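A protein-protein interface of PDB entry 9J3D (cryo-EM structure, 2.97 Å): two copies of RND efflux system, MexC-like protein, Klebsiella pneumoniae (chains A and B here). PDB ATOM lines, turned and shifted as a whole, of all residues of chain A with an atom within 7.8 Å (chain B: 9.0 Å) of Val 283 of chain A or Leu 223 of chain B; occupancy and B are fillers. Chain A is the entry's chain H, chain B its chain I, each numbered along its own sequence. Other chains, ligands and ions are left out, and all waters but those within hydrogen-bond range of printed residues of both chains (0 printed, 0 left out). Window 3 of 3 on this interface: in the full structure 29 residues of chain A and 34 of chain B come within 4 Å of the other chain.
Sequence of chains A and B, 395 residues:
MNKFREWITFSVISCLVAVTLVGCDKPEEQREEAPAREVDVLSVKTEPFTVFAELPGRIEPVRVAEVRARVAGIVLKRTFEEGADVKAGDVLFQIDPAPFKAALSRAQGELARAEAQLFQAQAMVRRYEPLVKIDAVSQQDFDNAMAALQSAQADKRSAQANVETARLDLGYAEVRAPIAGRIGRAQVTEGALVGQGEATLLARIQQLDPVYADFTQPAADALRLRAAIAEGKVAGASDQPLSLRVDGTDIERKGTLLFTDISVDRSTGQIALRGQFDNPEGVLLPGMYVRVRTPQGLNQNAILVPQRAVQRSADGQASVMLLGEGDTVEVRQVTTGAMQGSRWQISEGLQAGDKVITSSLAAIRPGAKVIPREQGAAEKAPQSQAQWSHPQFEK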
ATOM      1  N   ILE A  59     -16.635  -1.013  17.553  1.00  0.00           N
ATOM      2  CA  ILE A  59     -15.612  -0.985  18.588  1.00  0.00           C
ATOM      3  C   ILE A  59     -14.556   0.049  18.228  1.00  0.00           C
ATOM      4  O   ILE A  59     -14.061   0.088  17.095  1.00  0.00           O
ATOM      5  CB  ILE A  59     -14.989  -2.376  18.765  1.00  0.00           C
ATOM      6  CG1 ILE A  59     -16.043  -3.375  19.237  1.00  0.00           C
ATOM      7  CG2 ILE A  59     -13.838  -2.323  19.748  1.00  0.00           C
ATOM      8  CD1 ILE A  59     -16.680  -3.005  20.550  1.00  0.00           C
ATOM      9  N   LEU A 208      -5.885  -1.029  23.504  1.00  0.00           N
ATOM     10  CA  LEU A 208      -6.861  -2.094  23.325  1.00  0.00           C
ATOM     11  C   LEU A 208      -7.629  -2.447  24.592  1.00  0.00           C
ATOM     12  O   LEU A 208      -8.514  -3.306  24.537  1.00  0.00           O
ATOM     13  CB  LEU A 208      -6.169  -3.350  22.783  1.00  0.00           C
ATOM     14  CG  LEU A 208      -4.721  -3.581  23.222  1.00  0.00           C
ATOM     15  CD1 LEU A 208      -4.648  -4.043  24.671  1.00  0.00           C
ATOM     16  CD2 LEU A 208      -4.032  -4.577  22.303  1.00  0.00           C
ATOM     17  N   VAL A 211     -12.031  -0.822  25.847  1.00  0.00           N
ATOM     18  CA  VAL A 211     -12.431  -0.309  24.546  1.00  0.00           C
ATOM     19  C   VAL A 211     -13.767   0.402  24.694  1.00  0.00           C
ATOM     20  O   VAL A 211     -14.479   0.242  25.688  1.00  0.00           O
ATOM     21  CB  VAL A 211     -12.525  -1.418  23.479  1.00  0.00           C
ATOM     22  CG1 VAL A 211     -11.147  -1.957  23.153  1.00  0.00           C
ATOM     23  CG2 VAL A 211     -13.431  -2.532  23.958  1.00  0.00           C
ATOM     24  N   VAL A 246     -20.622  -9.927  19.727  1.00  0.00           N
ATOM     25  CA  VAL A 246     -19.985  -9.867  18.419  1.00  0.00           C
ATOM     26  C   VAL A 246     -20.797 -10.711  17.450  1.00  0.00           C
ATOM     27  O   VAL A 246     -21.140 -11.861  17.748  1.00  0.00           O
ATOM     28  CB  VAL A 246     -18.530 -10.354  18.500  1.00  0.00           C
ATOM     29  CG1 VAL A 246     -17.917 -10.427  17.114  1.00  0.00           C
ATOM     30  CG2 VAL A 246     -17.718  -9.442  19.401  1.00  0.00           C
ATOM     31  N   ASP A 247     -21.117 -10.139  16.292  1.00  0.00           N
ATOM     32  CA  ASP A 247     -21.968 -10.827  15.332  1.00  0.00           C
ATOM     33  C   ASP A 247     -21.293 -12.092  14.817  1.00  0.00           C
ATOM     34  O   ASP A 247     -20.106 -12.094  14.481  1.00  0.00           O
ATOM     35  CB  ASP A 247     -22.306  -9.896  14.169  1.00  0.00           C
ATOM     36  CG  ASP A 247     -23.710 -10.108  13.646  1.00  0.00           C
ATOM     37  OD1 ASP A 247     -24.382 -11.055  14.102  1.00  0.00           O
ATOM     38  OD2 ASP A 247     -24.147  -9.320  12.783  1.00  0.00           O
ATOM     39  N   GLY A 248     -22.061 -13.177  14.758  1.00  0.00           N
ATOM     40  CA  GLY A 248     -21.541 -14.446  14.299  1.00  0.00           C
ATOM     41  C   GLY A 248     -20.791 -15.249  15.334  1.00  0.00           C
ATOM     42  O   GLY A 248     -20.311 -16.341  15.019  1.00  0.00           O
ATOM     43  N   THR A 249     -20.669 -14.746  16.561  1.00  0.00           N
ATOM     44  CA  THR A 249     -19.971 -15.444  17.631  1.00  0.00           C
ATOM     45  C   THR A 249     -20.831 -15.448  18.885  1.00  0.00           C
ATOM     46  O   THR A 249     -21.851 -14.761  18.970  1.00  0.00           O
ATOM     47  CB  THR A 249     -18.613 -14.801  17.952  1.00  0.00           C
ATOM     48  OG1 THR A 249     -18.819 -13.614  18.727  1.00  0.00           O
ATOM     49  CG2 THR A 249     -17.859 -14.446  16.678  1.00  0.00           C
ATOM     50  N   ILE A 251     -19.384 -14.590  21.769  1.00  0.00           N
ATOM     51  CA  ILE A 251     -18.586 -13.777  22.682  1.00  0.00           C
ATOM     52  C   ILE A 251     -19.473 -12.669  23.241  1.00  0.00           C
ATOM     53  O   ILE A 251     -19.956 -11.813  22.494  1.00  0.00           O
ATOM     54  CB  ILE A 251     -17.353 -13.202  21.981  1.00  0.00           C
ATOM     55  CG1 ILE A 251     -16.512 -14.331  21.385  1.00  0.00           C
ATOM     56  CG2 ILE A 251     -16.530 -12.373  22.947  1.00  0.00           C
ATOM     57  CD1 ILE A 251     -15.444 -13.858  20.434  1.00  0.00           C
ATOM     58  N   ARG A 253     -19.799  -9.621  26.317  1.00  0.00           N
ATOM     59  CA  ARG A 253     -19.049  -8.786  27.244  1.00  0.00           C
ATOM     60  C   ARG A 253     -19.989  -7.802  27.926  1.00  0.00           C
ATOM     61  O   ARG A 253     -20.918  -7.288  27.303  1.00  0.00           O
ATOM     62  CB  ARG A 253     -17.932  -8.026  26.523  1.00  0.00           C
ATOM     63  CG  ARG A 253     -16.808  -8.904  26.001  1.00  0.00           C
ATOM     64  CD  ARG A 253     -16.028  -9.547  27.133  1.00  0.00           C
ATOM     65  NE  ARG A 253     -14.809 -10.187  26.655  1.00  0.00           N
ATOM     66  CZ  ARG A 253     -14.744 -11.434  26.211  1.00  0.00           C
ATOM     67  NH1 ARG A 253     -15.812 -12.214  26.180  1.00  0.00           N
ATOM     68  NH2 ARG A 253     -13.577 -11.911  25.787  1.00  0.00           N
ATOM     69  N   ASP A 278     -14.640  -3.812  29.025  1.00  0.00           N
ATOM     70  CA  ASP A 278     -13.327  -4.367  29.327  1.00  0.00           C
ATOM     71  C   ASP A 278     -12.908  -5.351  28.244  1.00  0.00           C
ATOM     72  O   ASP A 278     -13.726  -6.117  27.728  1.00  0.00           O
ATOM     73  CB  ASP A 278     -13.340  -5.062  30.687  1.00  0.00           C
ATOM     74  CG  ASP A 278     -13.691  -4.120  31.820  1.00  0.00           C
ATOM     75  OD1 ASP A 278     -13.463  -2.901  31.675  1.00  0.00           O
ATOM     76  OD2 ASP A 278     -14.198  -4.599  32.856  1.00  0.00           O
ATOM     77  N   ASN A 279     -11.625  -5.326  27.894  1.00  0.00           N
ATOM     78  CA  ASN A 279     -11.074  -6.212  26.869  1.00  0.00           C
ATOM     79  C   ASN A 279      -9.692  -6.688  27.297  1.00  0.00           C
ATOM     80  O   ASN A 279      -8.675  -6.294  26.721  1.00  0.00           O
ATOM     81  CB  ASN A 279     -11.029  -5.498  25.519  1.00  0.00           C
ATOM     82  CG  ASN A 279     -10.609  -6.409  24.390  1.00  0.00           C
ATOM     83  OD1 ASN A 279     -10.972  -7.583  24.356  1.00  0.00           O
ATOM     84  ND2 ASN A 279      -9.851  -5.866  23.447  1.00  0.00           N
ATOM     85  N   PRO A 280      -9.620  -7.542  28.320  1.00  0.00           N
ATOM     86  CA  PRO A 280      -8.302  -7.992  28.795  1.00  0.00           C
ATOM     87  C   PRO A 280      -7.602  -8.935  27.835  1.00  0.00           C
ATOM     88  O   PRO A 280      -6.369  -8.898  27.733  1.00  0.00           O
ATOM     89  CB  PRO A 280      -8.631  -8.681  30.125  1.00  0.00           C
ATOM     90  CG  PRO A 280     -10.023  -9.164  29.948  1.00  0.00           C
ATOM     91  CD  PRO A 280     -10.719  -8.138  29.099  1.00  0.00           C
ATOM     92  N   GLU A 281      -8.346  -9.780  27.126  1.00  0.00           N
ATOM     93  CA  GLU A 281      -7.740 -10.731  26.206  1.00  0.00           C
ATOM     94  C   GLU A 281      -7.464 -10.139  24.832  1.00  0.00           C
ATOM     95  O   GLU A 281      -6.811 -10.794  24.015  1.00  0.00           O
ATOM     96  CB  GLU A 281      -8.634 -11.963  26.055  1.00  0.00           C
ATOM     97  CG  GLU A 281      -8.991 -12.646  27.363  1.00  0.00           C
ATOM     98  CD  GLU A 281     -10.231 -12.060  28.007  1.00  0.00           C
ATOM     99  OE1 GLU A 281     -10.968 -11.324  27.318  1.00  0.00           O
ATOM    100  OE2 GLU A 281     -10.471 -12.335  29.202  1.00  0.00           O
ATOM    101  N   GLY A 282      -7.939  -8.927  24.555  1.00  0.00           N
ATOM    102  CA  GLY A 282      -7.757  -8.353  23.239  1.00  0.00           C
ATOM    103  C   GLY A 282      -8.644  -8.946  22.171  1.00  0.00           C
ATOM    104  O   GLY A 282      -8.348  -8.801  20.984  1.00  0.00           O
ATOM    105  N   VAL A 283      -9.726  -9.621  22.562  1.00  0.00           N
ATOM    106  CA  VAL A 283     -10.625 -10.216  21.580  1.00  0.00           C
ATOM    107  C   VAL A 283     -11.395  -9.146  20.816  1.00  0.00           C
ATOM    108  O   VAL A 283     -11.518  -9.224  19.588  1.00  0.00           O
ATOM    109  CB  VAL A 283     -11.579 -11.204  22.268  1.00  0.00           C
ATOM    110  CG1 VAL A 283     -12.553 -11.784  21.262  1.00  0.00           C
ATOM    111  CG2 VAL A 283     -10.791 -12.307  22.954  1.00  0.00           C
ATOM    112  N   LEU A 284     -11.918  -8.141  21.510  1.00  0.00           N
ATOM    113  CA  LEU A 284     -12.679  -7.075  20.869  1.00  0.00           C
ATOM    114  C   LEU A 284     -11.726  -6.194  20.073  1.00  0.00           C
ATOM    115  O   LEU A 284     -10.906  -5.472  20.652  1.00  0.00           O
ATOM    116  CB  LEU A 284     -13.438  -6.264  21.915  1.00  0.00           C
ATOM    117  CG  LEU A 284     -14.398  -7.060  22.797  1.00  0.00           C
ATOM    118  CD1 LEU A 284     -15.090  -6.151  23.798  1.00  0.00           C
ATOM    119  CD2 LEU A 284     -15.415  -7.795  21.944  1.00  0.00           C
ATOM    120  N   LEU A 285     -11.841  -6.245  18.743  1.00  0.00           N
ATOM    121  CA  LEU A 285     -10.929  -5.489  17.906  1.00  0.00           C
ATOM    122  C   LEU A 285     -11.606  -4.212  17.417  1.00  0.00           C
ATOM    123  O   LEU A 285     -12.819  -4.209  17.174  1.00  0.00           O
ATOM    124  CB  LEU A 285     -10.495  -6.301  16.687  1.00  0.00           C
ATOM    125  CG  LEU A 285      -9.872  -7.664  16.976  1.00  0.00           C
ATOM    126  CD1 LEU A 285      -9.448  -8.388  15.726  1.00  0.00           C
ATOM    127  CD2 LEU A 285      -8.837  -7.625  17.918  1.00  0.00           C
ATOM    128  N   PRO A 286     -10.856  -3.124  17.268  1.00  0.00           N
ATOM    129  CA  PRO A 286     -11.449  -1.873  16.783  1.00  0.00           C
ATOM    130  C   PRO A 286     -12.040  -2.032  15.391  1.00  0.00           C
ATOM    131  O   PRO A 286     -11.497  -2.739  14.541  1.00  0.00           O
ATOM    132  CB  PRO A 286     -10.262  -0.907  16.785  1.00  0.00           C
ATOM    133  CG  PRO A 286      -9.358  -1.445  17.831  1.00  0.00           C
ATOM    134  CD  PRO A 286      -9.467  -2.935  17.710  1.00  0.00           C
ATOM    135  N   MET A 288     -14.804  -3.536  14.582  1.00  0.00           N
ATOM    136  CA  MET A 288     -15.706  -4.669  14.445  1.00  0.00           C
ATOM    137  C   MET A 288     -17.144  -4.223  14.684  1.00  0.00           C
ATOM    138  O   MET A 288     -17.429  -3.479  15.624  1.00  0.00           O
ATOM    139  CB  MET A 288     -15.320  -5.765  15.442  1.00  0.00           C
ATOM    140  CG  MET A 288     -14.629  -6.988  14.842  1.00  0.00           C
ATOM    141  SD  MET A 288     -15.493  -7.921  13.560  1.00  0.00           S
ATOM    142  CE  MET A 288     -17.197  -7.821  14.093  1.00  0.00           C
ATOM    143  N   GLN B 217      -7.901 -11.346   5.434  1.00  0.00           N
ATOM    144  CA  GLN B 217      -8.677 -12.448   5.988  1.00  0.00           C
ATOM    145  C   GLN B 217      -9.902 -11.924   6.725  1.00  0.00           C
ATOM    146  O   GLN B 217      -9.816 -10.907   7.418  1.00  0.00           O
ATOM    147  CB  GLN B 217      -7.830 -13.285   6.957  1.00  0.00           C
ATOM    148  CG  GLN B 217      -8.517 -14.535   7.480  1.00  0.00           C
ATOM    149  CD  GLN B 217      -7.664 -15.301   8.472  1.00  0.00           C
ATOM    150  OE1 GLN B 217      -6.726 -14.755   9.051  1.00  0.00           O
ATOM    151  NE2 GLN B 217      -7.987 -16.572   8.672  1.00  0.00           N
ATOM    152  N   PRO B 218     -11.045 -12.600   6.611  1.00  0.00           N
ATOM    153  CA  PRO B 218     -12.232 -12.176   7.368  1.00  0.00           C
ATOM    154  C   PRO B 218     -11.981 -12.201   8.870  1.00  0.00           C
ATOM    155  O   PRO B 218     -11.303 -13.089   9.391  1.00  0.00           O
ATOM    156  CB  PRO B 218     -13.295 -13.198   6.955  1.00  0.00           C
ATOM    157  CG  PRO B 218     -12.859 -13.658   5.614  1.00  0.00           C
ATOM    158  CD  PRO B 218     -11.361 -13.677   5.659  1.00  0.00           C
ATOM    159  N   ALA B 219     -12.538 -11.207   9.565  1.00  0.00           N
ATOM    160  CA  ALA B 219     -12.350 -11.117  11.008  1.00  0.00           C
ATOM    161  C   ALA B 219     -13.081 -12.230  11.742  1.00  0.00           C
ATOM    162  O   ALA B 219     -12.596 -12.718  12.768  1.00  0.00           O
ATOM    163  CB  ALA B 219     -12.815  -9.754  11.515  1.00  0.00           C
ATOM    164  N   ALA B 220     -14.250 -12.634  11.243  1.00  0.00           N
ATOM    165  CA  ALA B 220     -14.990 -13.715  11.885  1.00  0.00           C
ATOM    166  C   ALA B 220     -14.206 -15.019  11.842  1.00  0.00           C
ATOM    167  O   ALA B 220     -14.193 -15.777  12.820  1.00  0.00           O
ATOM    168  CB  ALA B 220     -16.354 -13.885  11.221  1.00  0.00           C
ATOM    169  N   ASP B 221     -13.550 -15.302  10.716  1.00  0.00           N
ATOM    170  CA  ASP B 221     -12.740 -16.511  10.617  1.00  0.00           C
ATOM    171  C   ASP B 221     -11.570 -16.472  11.592  1.00  0.00           C
ATOM    172  O   ASP B 221     -11.248 -17.483  12.224  1.00  0.00           O
ATOM    173  CB  ASP B 221     -12.241 -16.691   9.186  1.00  0.00           C
ATOM    174  CG  ASP B 221     -13.372 -16.900   8.198  1.00  0.00           C
ATOM    175  OD1 ASP B 221     -14.501 -17.194   8.641  1.00  0.00           O
ATOM    176  OD2 ASP B 221     -13.131 -16.769   6.979  1.00  0.00           O
ATOM    177  N   ALA B 222     -10.921 -15.313  11.722  1.00  0.00           N
ATOM    178  CA  ALA B 222      -9.824 -15.187  12.674  1.00  0.00           C
ATOM    179  C   ALA B 222     -10.311 -15.380  14.104  1.00  0.00           C
ATOM    180  O   ALA B 222      -9.643 -16.033  14.914  1.00  0.00           O
ATOM    181  CB  ALA B 222      -9.144 -13.829  12.516  1.00  0.00           C
ATOM    182  N   LEU B 223     -11.474 -14.818  14.434  1.00  0.00           N
ATOM    183  CA  LEU B 223     -12.027 -14.998  15.771  1.00  0.00           C
ATOM    184  C   LEU B 223     -12.376 -16.457  16.033  1.00  0.00           C
ATOM    185  O   LEU B 223     -12.152 -16.963  17.138  1.00  0.00           O
ATOM    186  CB  LEU B 223     -13.254 -14.110  15.955  1.00  0.00           C
ATOM    187  CG  LEU B 223     -12.971 -12.624  16.173  1.00  0.00           C
ATOM    188  CD1 LEU B 223     -14.267 -11.830  16.212  1.00  0.00           C
ATOM    189  CD2 LEU B 223     -12.175 -12.417  17.447  1.00  0.00           C
ATOM    190  N   ARG B 224     -12.935 -17.146  15.037  1.00  0.00           N
ATOM    191  CA  ARG B 224     -13.246 -18.562  15.203  1.00  0.00           C
ATOM    192  C   ARG B 224     -11.980 -19.386  15.401  1.00  0.00           C
ATOM    193  O   ARG B 224     -11.945 -20.291  16.242  1.00  0.00           O
ATOM    194  CB  ARG B 224     -14.034 -19.070  13.997  1.00  0.00           C
ATOM    195  CG  ARG B 224     -15.475 -18.594  13.953  1.00  0.00           C
ATOM    196  CD  ARG B 224     -16.229 -19.237  12.805  1.00  0.00           C
ATOM    197  NE  ARG B 224     -17.156 -18.304  12.176  1.00  0.00           N
ATOM    198  CZ  ARG B 224     -17.083 -17.914  10.912  1.00  0.00           C
ATOM    199  NH1 ARG B 224     -16.134 -18.360  10.105  1.00  0.00           N
ATOM    200  NH2 ARG B 224     -17.985 -17.057  10.444  1.00  0.00           N
ATOM    201  N   LEU B 225     -10.930 -19.088  14.633  1.00  0.00           N
ATOM    202  CA  LEU B 225      -9.660 -19.784  14.809  1.00  0.00           C
ATOM    203  C   LEU B 225      -9.093 -19.539  16.201  1.00  0.00           C
ATOM    204  O   LEU B 225      -8.598 -20.463  16.855  1.00  0.00           O
ATOM    205  CB  LEU B 225      -8.667 -19.336  13.737  1.00  0.00           C
ATOM    206  CG  LEU B 225      -7.211 -19.760  13.929  1.00  0.00           C
ATOM    207  CD1 LEU B 225      -7.089 -21.271  13.974  1.00  0.00           C
ATOM    208  CD2 LEU B 225      -6.333 -19.177  12.833  1.00  0.00           C
ATOM    209  N   ARG B 226      -9.160 -18.292  16.671  1.00  0.00           N
ATOM    210  CA  ARG B 226      -8.652 -17.974  18.000  1.00  0.00           C
ATOM    211  C   ARG B 226      -9.452 -18.686  19.083  1.00  0.00           C
ATOM    212  O   ARG B 226      -8.884 -19.167  20.069  1.00  0.00           O
ATOM    213  CB  ARG B 226      -8.676 -16.464  18.220  1.00  0.00           C
ATOM    214  CG  ARG B 226      -8.097 -16.017  19.547  1.00  0.00           C
ATOM    215  CD  ARG B 226      -8.107 -14.504  19.659  1.00  0.00           C
ATOM    216  NE  ARG B 226      -7.685 -14.054  20.980  1.00  0.00           N
ATOM    217  CZ  ARG B 226      -7.511 -12.784  21.317  1.00  0.00           C
ATOM    218  NH1 ARG B 226      -7.720 -11.805  20.453  1.00  0.00           N
ATOM    219  NH2 ARG B 226      -7.119 -12.489  22.554  1.00  0.00           N
ATOM    220  N   ALA B 227     -10.774 -18.753  18.924  1.00  0.00           N
ATOM    221  CA  ALA B 227     -11.606 -19.454  19.897  1.00  0.00           C
ATOM    222  C   ALA B 227     -11.292 -20.944  19.909  1.00  0.00           C
ATOM    223  O   ALA B 227     -11.234 -21.570  20.974  1.00  0.00           O
ATOM    224  CB  ALA B 227     -13.083 -19.214  19.592  1.00  0.00           C
ATOM    225  N   ALA B 228     -11.094 -21.532  18.728  1.00  0.00           N
ATOM    226  CA  ALA B 228     -10.739 -22.946  18.661  1.00  0.00           C
ATOM    227  C   ALA B 228      -9.373 -23.206  19.280  1.00  0.00           C
ATOM    228  O   ALA B 228      -9.162 -24.260  19.891  1.00  0.00           O
ATOM    229  CB  ALA B 228     -10.773 -23.428  17.213  1.00  0.00           C
ATOM    230  N   ILE B 229      -8.435 -22.273  19.124  1.00  0.00           N
ATOM    231  CA  ILE B 229      -7.143 -22.398  19.790  1.00  0.00           C
ATOM    232  C   ILE B 229      -7.316 -22.325  21.303  1.00  0.00           C
ATOM    233  O   ILE B 229      -6.750 -23.132  22.050  1.00  0.00           O
ATOM    234  CB  ILE B 229      -6.170 -21.317  19.285  1.00  0.00           C
ATOM    235  CG1 ILE B 229      -5.771 -21.587  17.835  1.00  0.00           C
ATOM    236  CG2 ILE B 229      -4.938 -21.248  20.173  1.00  0.00           C
ATOM    237  CD1 ILE B 229      -5.093 -20.414  17.165  1.00  0.00           C
ATOM    238  N   ALA B 230      -8.104 -21.356  21.774  1.00  0.00           N
ATOM    239  CA  ALA B 230      -8.317 -21.199  23.209  1.00  0.00           C
ATOM    240  C   ALA B 230      -9.020 -22.407  23.806  1.00  0.00           C
ATOM    241  O   ALA B 230      -8.656 -22.859  24.897  1.00  0.00           O
ATOM    242  CB  ALA B 230      -9.118 -19.928  23.486  1.00  0.00           C
ATOM    243  N   GLU B 231     -10.026 -22.937  23.117  1.00  0.00           N
ATOM    244  CA  GLU B 231     -10.666 -24.160  23.570  1.00  0.00           C
ATOM    245  C   GLU B 231      -9.741 -25.364  23.472  1.00  0.00           C
ATOM    246  O   GLU B 231      -9.955 -26.343  24.192  1.00  0.00           O
ATOM    247  CB  GLU B 231     -11.958 -24.403  22.781  1.00  0.00           C
ATOM    248  CG  GLU B 231     -13.058 -23.394  23.102  1.00  0.00           C
ATOM    249  CD  GLU B 231     -14.275 -23.525  22.205  1.00  0.00           C
ATOM    250  OE1 GLU B 231     -14.461 -24.598  21.596  1.00  0.00           O
ATOM    251  OE2 GLU B 231     -15.049 -22.549  22.111  1.00  0.00           O
ATOM    252  N   VAL B 234      -7.813 -26.850  18.120  1.00  0.00           N
ATOM    253  CA  VAL B 234      -6.774 -26.733  17.106  1.00  0.00           C
ATOM    254  C   VAL B 234      -5.547 -26.100  17.743  1.00  0.00           C
ATOM    255  O   VAL B 234      -5.666 -25.305  18.683  1.00  0.00           O
ATOM    256  CB  VAL B 234      -7.240 -25.908  15.886  1.00  0.00           C
ATOM    257  CG1 VAL B 234      -8.529 -26.478  15.312  1.00  0.00           C
ATOM    258  CG2 VAL B 234      -7.423 -24.447  16.257  1.00  0.00           C
ATOM    259  N   ILE B 262      -4.541  -5.535  14.139  1.00  0.00           N
ATOM    260  CA  ILE B 262      -5.499  -5.518  15.242  1.00  0.00           C
ATOM    261  C   ILE B 262      -6.783  -4.798  14.847  1.00  0.00           C
ATOM    262  O   ILE B 262      -7.835  -5.034  15.460  1.00  0.00           O
ATOM    263  CB  ILE B 262      -4.861  -4.825  16.468  1.00  0.00           C
ATOM    264  CG1 ILE B 262      -5.796  -4.676  17.654  1.00  0.00           C
ATOM    265  CG2 ILE B 262      -4.274  -3.489  16.118  1.00  0.00           C
ATOM    266  CD1 ILE B 262      -6.276  -5.862  18.026  1.00  0.00           C
ATOM    267  N   VAL B 264      -9.971  -3.619  12.297  1.00  0.00           N
ATOM    268  CA  VAL B 264     -10.856  -4.201  11.295  1.00  0.00           C
ATOM    269  C   VAL B 264     -11.229  -3.115  10.297  1.00  0.00           C
ATOM    270  O   VAL B 264     -11.616  -2.009  10.690  1.00  0.00           O
ATOM    271  CB  VAL B 264     -12.111  -4.804  11.950  1.00  0.00           C
ATOM    272  CG1 VAL B 264     -13.279  -4.797  10.982  1.00  0.00           C
ATOM    273  CG2 VAL B 264     -11.830  -6.211  12.439  1.00  0.00           C
ATOM    274  N   GLY B 269     -14.973  -5.175   6.812  1.00  0.00           N
ATOM    275  CA  GLY B 269     -14.986  -6.054   7.964  1.00  0.00           C
ATOM    276  C   GLY B 269     -13.961  -7.164   7.958  1.00  0.00           C
ATOM    277  O   GLY B 269     -14.212  -8.224   8.536  1.00  0.00           O
ATOM    278  N   ILE B 271      -9.584  -8.185   8.316  1.00  0.00           N
ATOM    279  CA  ILE B 271      -8.295  -7.753   8.840  1.00  0.00           C
ATOM    280  C   ILE B 271      -7.218  -7.997   7.796  1.00  0.00           C
ATOM    281  O   ILE B 271      -7.298  -8.935   6.991  1.00  0.00           O
ATOM    282  CB  ILE B 271      -7.965  -8.476  10.160  1.00  0.00           C
ATOM    283  CG1 ILE B 271      -7.884  -9.986   9.943  1.00  0.00           C
ATOM    284  CG2 ILE B 271      -8.998  -8.153  11.216  1.00  0.00           C
ATOM    285  CD1 ILE B 271      -7.281 -10.736  11.105  1.00  0.00           C
ATOM    286  N   GLN B 296      -4.457 -22.572   8.780  1.00  0.00           N
ATOM    287  CA  GLN B 296      -5.467 -22.241   9.777  1.00  0.00           C
ATOM    288  C   GLN B 296      -5.402 -23.146  11.001  1.00  0.00           C
ATOM    289  O   GLN B 296      -6.432 -23.395  11.640  1.00  0.00           O
ATOM    290  CB  GLN B 296      -6.860 -22.299   9.150  1.00  0.00           C
ATOM    291  CG  GLN B 296      -7.019 -21.424   7.925  1.00  0.00           C
ATOM    292  CD  GLN B 296      -6.738 -19.969   8.216  1.00  0.00           C
ATOM    293  OE1 GLN B 296      -7.376 -19.360   9.072  1.00  0.00           O
ATOM    294  NE2 GLN B 296      -5.773 -19.401   7.503  1.00  0.00           N
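N of Val 264 of chain B sits at hydrogen-bond distance from O of Pro 286 of chain A, at 2.9 Å.
O of Gly 282 of chain A sits at hydrogen-bond distance from NH1 of Arg 226 of chain B, 3.1 Å away.
O of Glu 281 of chain A sits close to NH2 of Arg 226 of chain B.
N of Ile 59 of chain A lies within hydrogen-bond range of O of Met 288 of chain A (3.2 Å).
OD1 of Asn 279 of chain A lies within hydrogen-bond range of N of Val 283 of chain A (3.0 Å).
N of Gly 282 of chain A lies within hydrogen-bond range of OD1 of Asn 279 of chain A, at 3.3 Å.
NH2 of Arg 253 of chain A is in salt-bridge range of OE1 of Glu 281 of chain A (3.1 Å).
Leu 223 of chain B touches Val 283 of chain A (CD2 to CG1, 3.9 Å).
Arg 226 of chain B touches Val 283 of chain A.
CD2 of Leu 285 of chain A touches CD1 of Ile 262 of chain B (3.1 Å).
Pro 286 of chain A touches Ile 262 of chain B (CD to O, 3.5 Å).
Met 288 of chain A touches Ala 219 of chain B (SD to CB, 3.8 Å).
CG of Met 288 of chain A touches CG2 of Val 264 of chain B, at 3.8 Å.
Asp 247 of chain A touches none of the printed residues of chain B.
Of chain B, only Arg 226 (3.1 Å) comes within 4 Å of Gly 282 of chain A.
Val 283 of chain A touches two residues of chain B.
Of the printed residues of chain B, Pro 286 of chain A touches Ile 262 and Val 264.
No residue of chain A comes within 4 Å of Ala 222 of chain B.
Of the printed residues of chain A, Leu 223 of chain B touches Val 283.
Of the printed residues of chain A, Arg 226 of chain B touches Glu 281 (2.3 Å), Gly 282 (3.1 Å) and Val 283 (3.5 Å).
The nearest printed residue of chain A that does not touch Leu 223 of chain B is Val 246 of chain A (4.01 Å).
The nearest printed residue of chain A that does not touch Arg 226 of chain B is Leu 285 of chain A (5.0 Å).
Printed residues of chain B that touch a printed residue of chain A: Ala 219, Leu 223, Arg 226, Ile 262 and Val 264.
Hydrophobic or aromatic side chains of chain B that line the printed part of chain A: Ala 219, Leu 223, Ile 262 and Val 264.
Of the 19 printed residues of chain A, 6 touch a printed residue of chain B.
Printed residues of chain A that touch a printed residue of chain B: Glu 281, Gly 282, Val 283, Leu 285, Pro 286 and Met 288.
Among the printed residues, 9 pairs touch across the chains.
No position is printed for both chains.
Of the 9 pairs that touch across the chains among the printed residues, none has its exchanged pair printed and touching as well.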
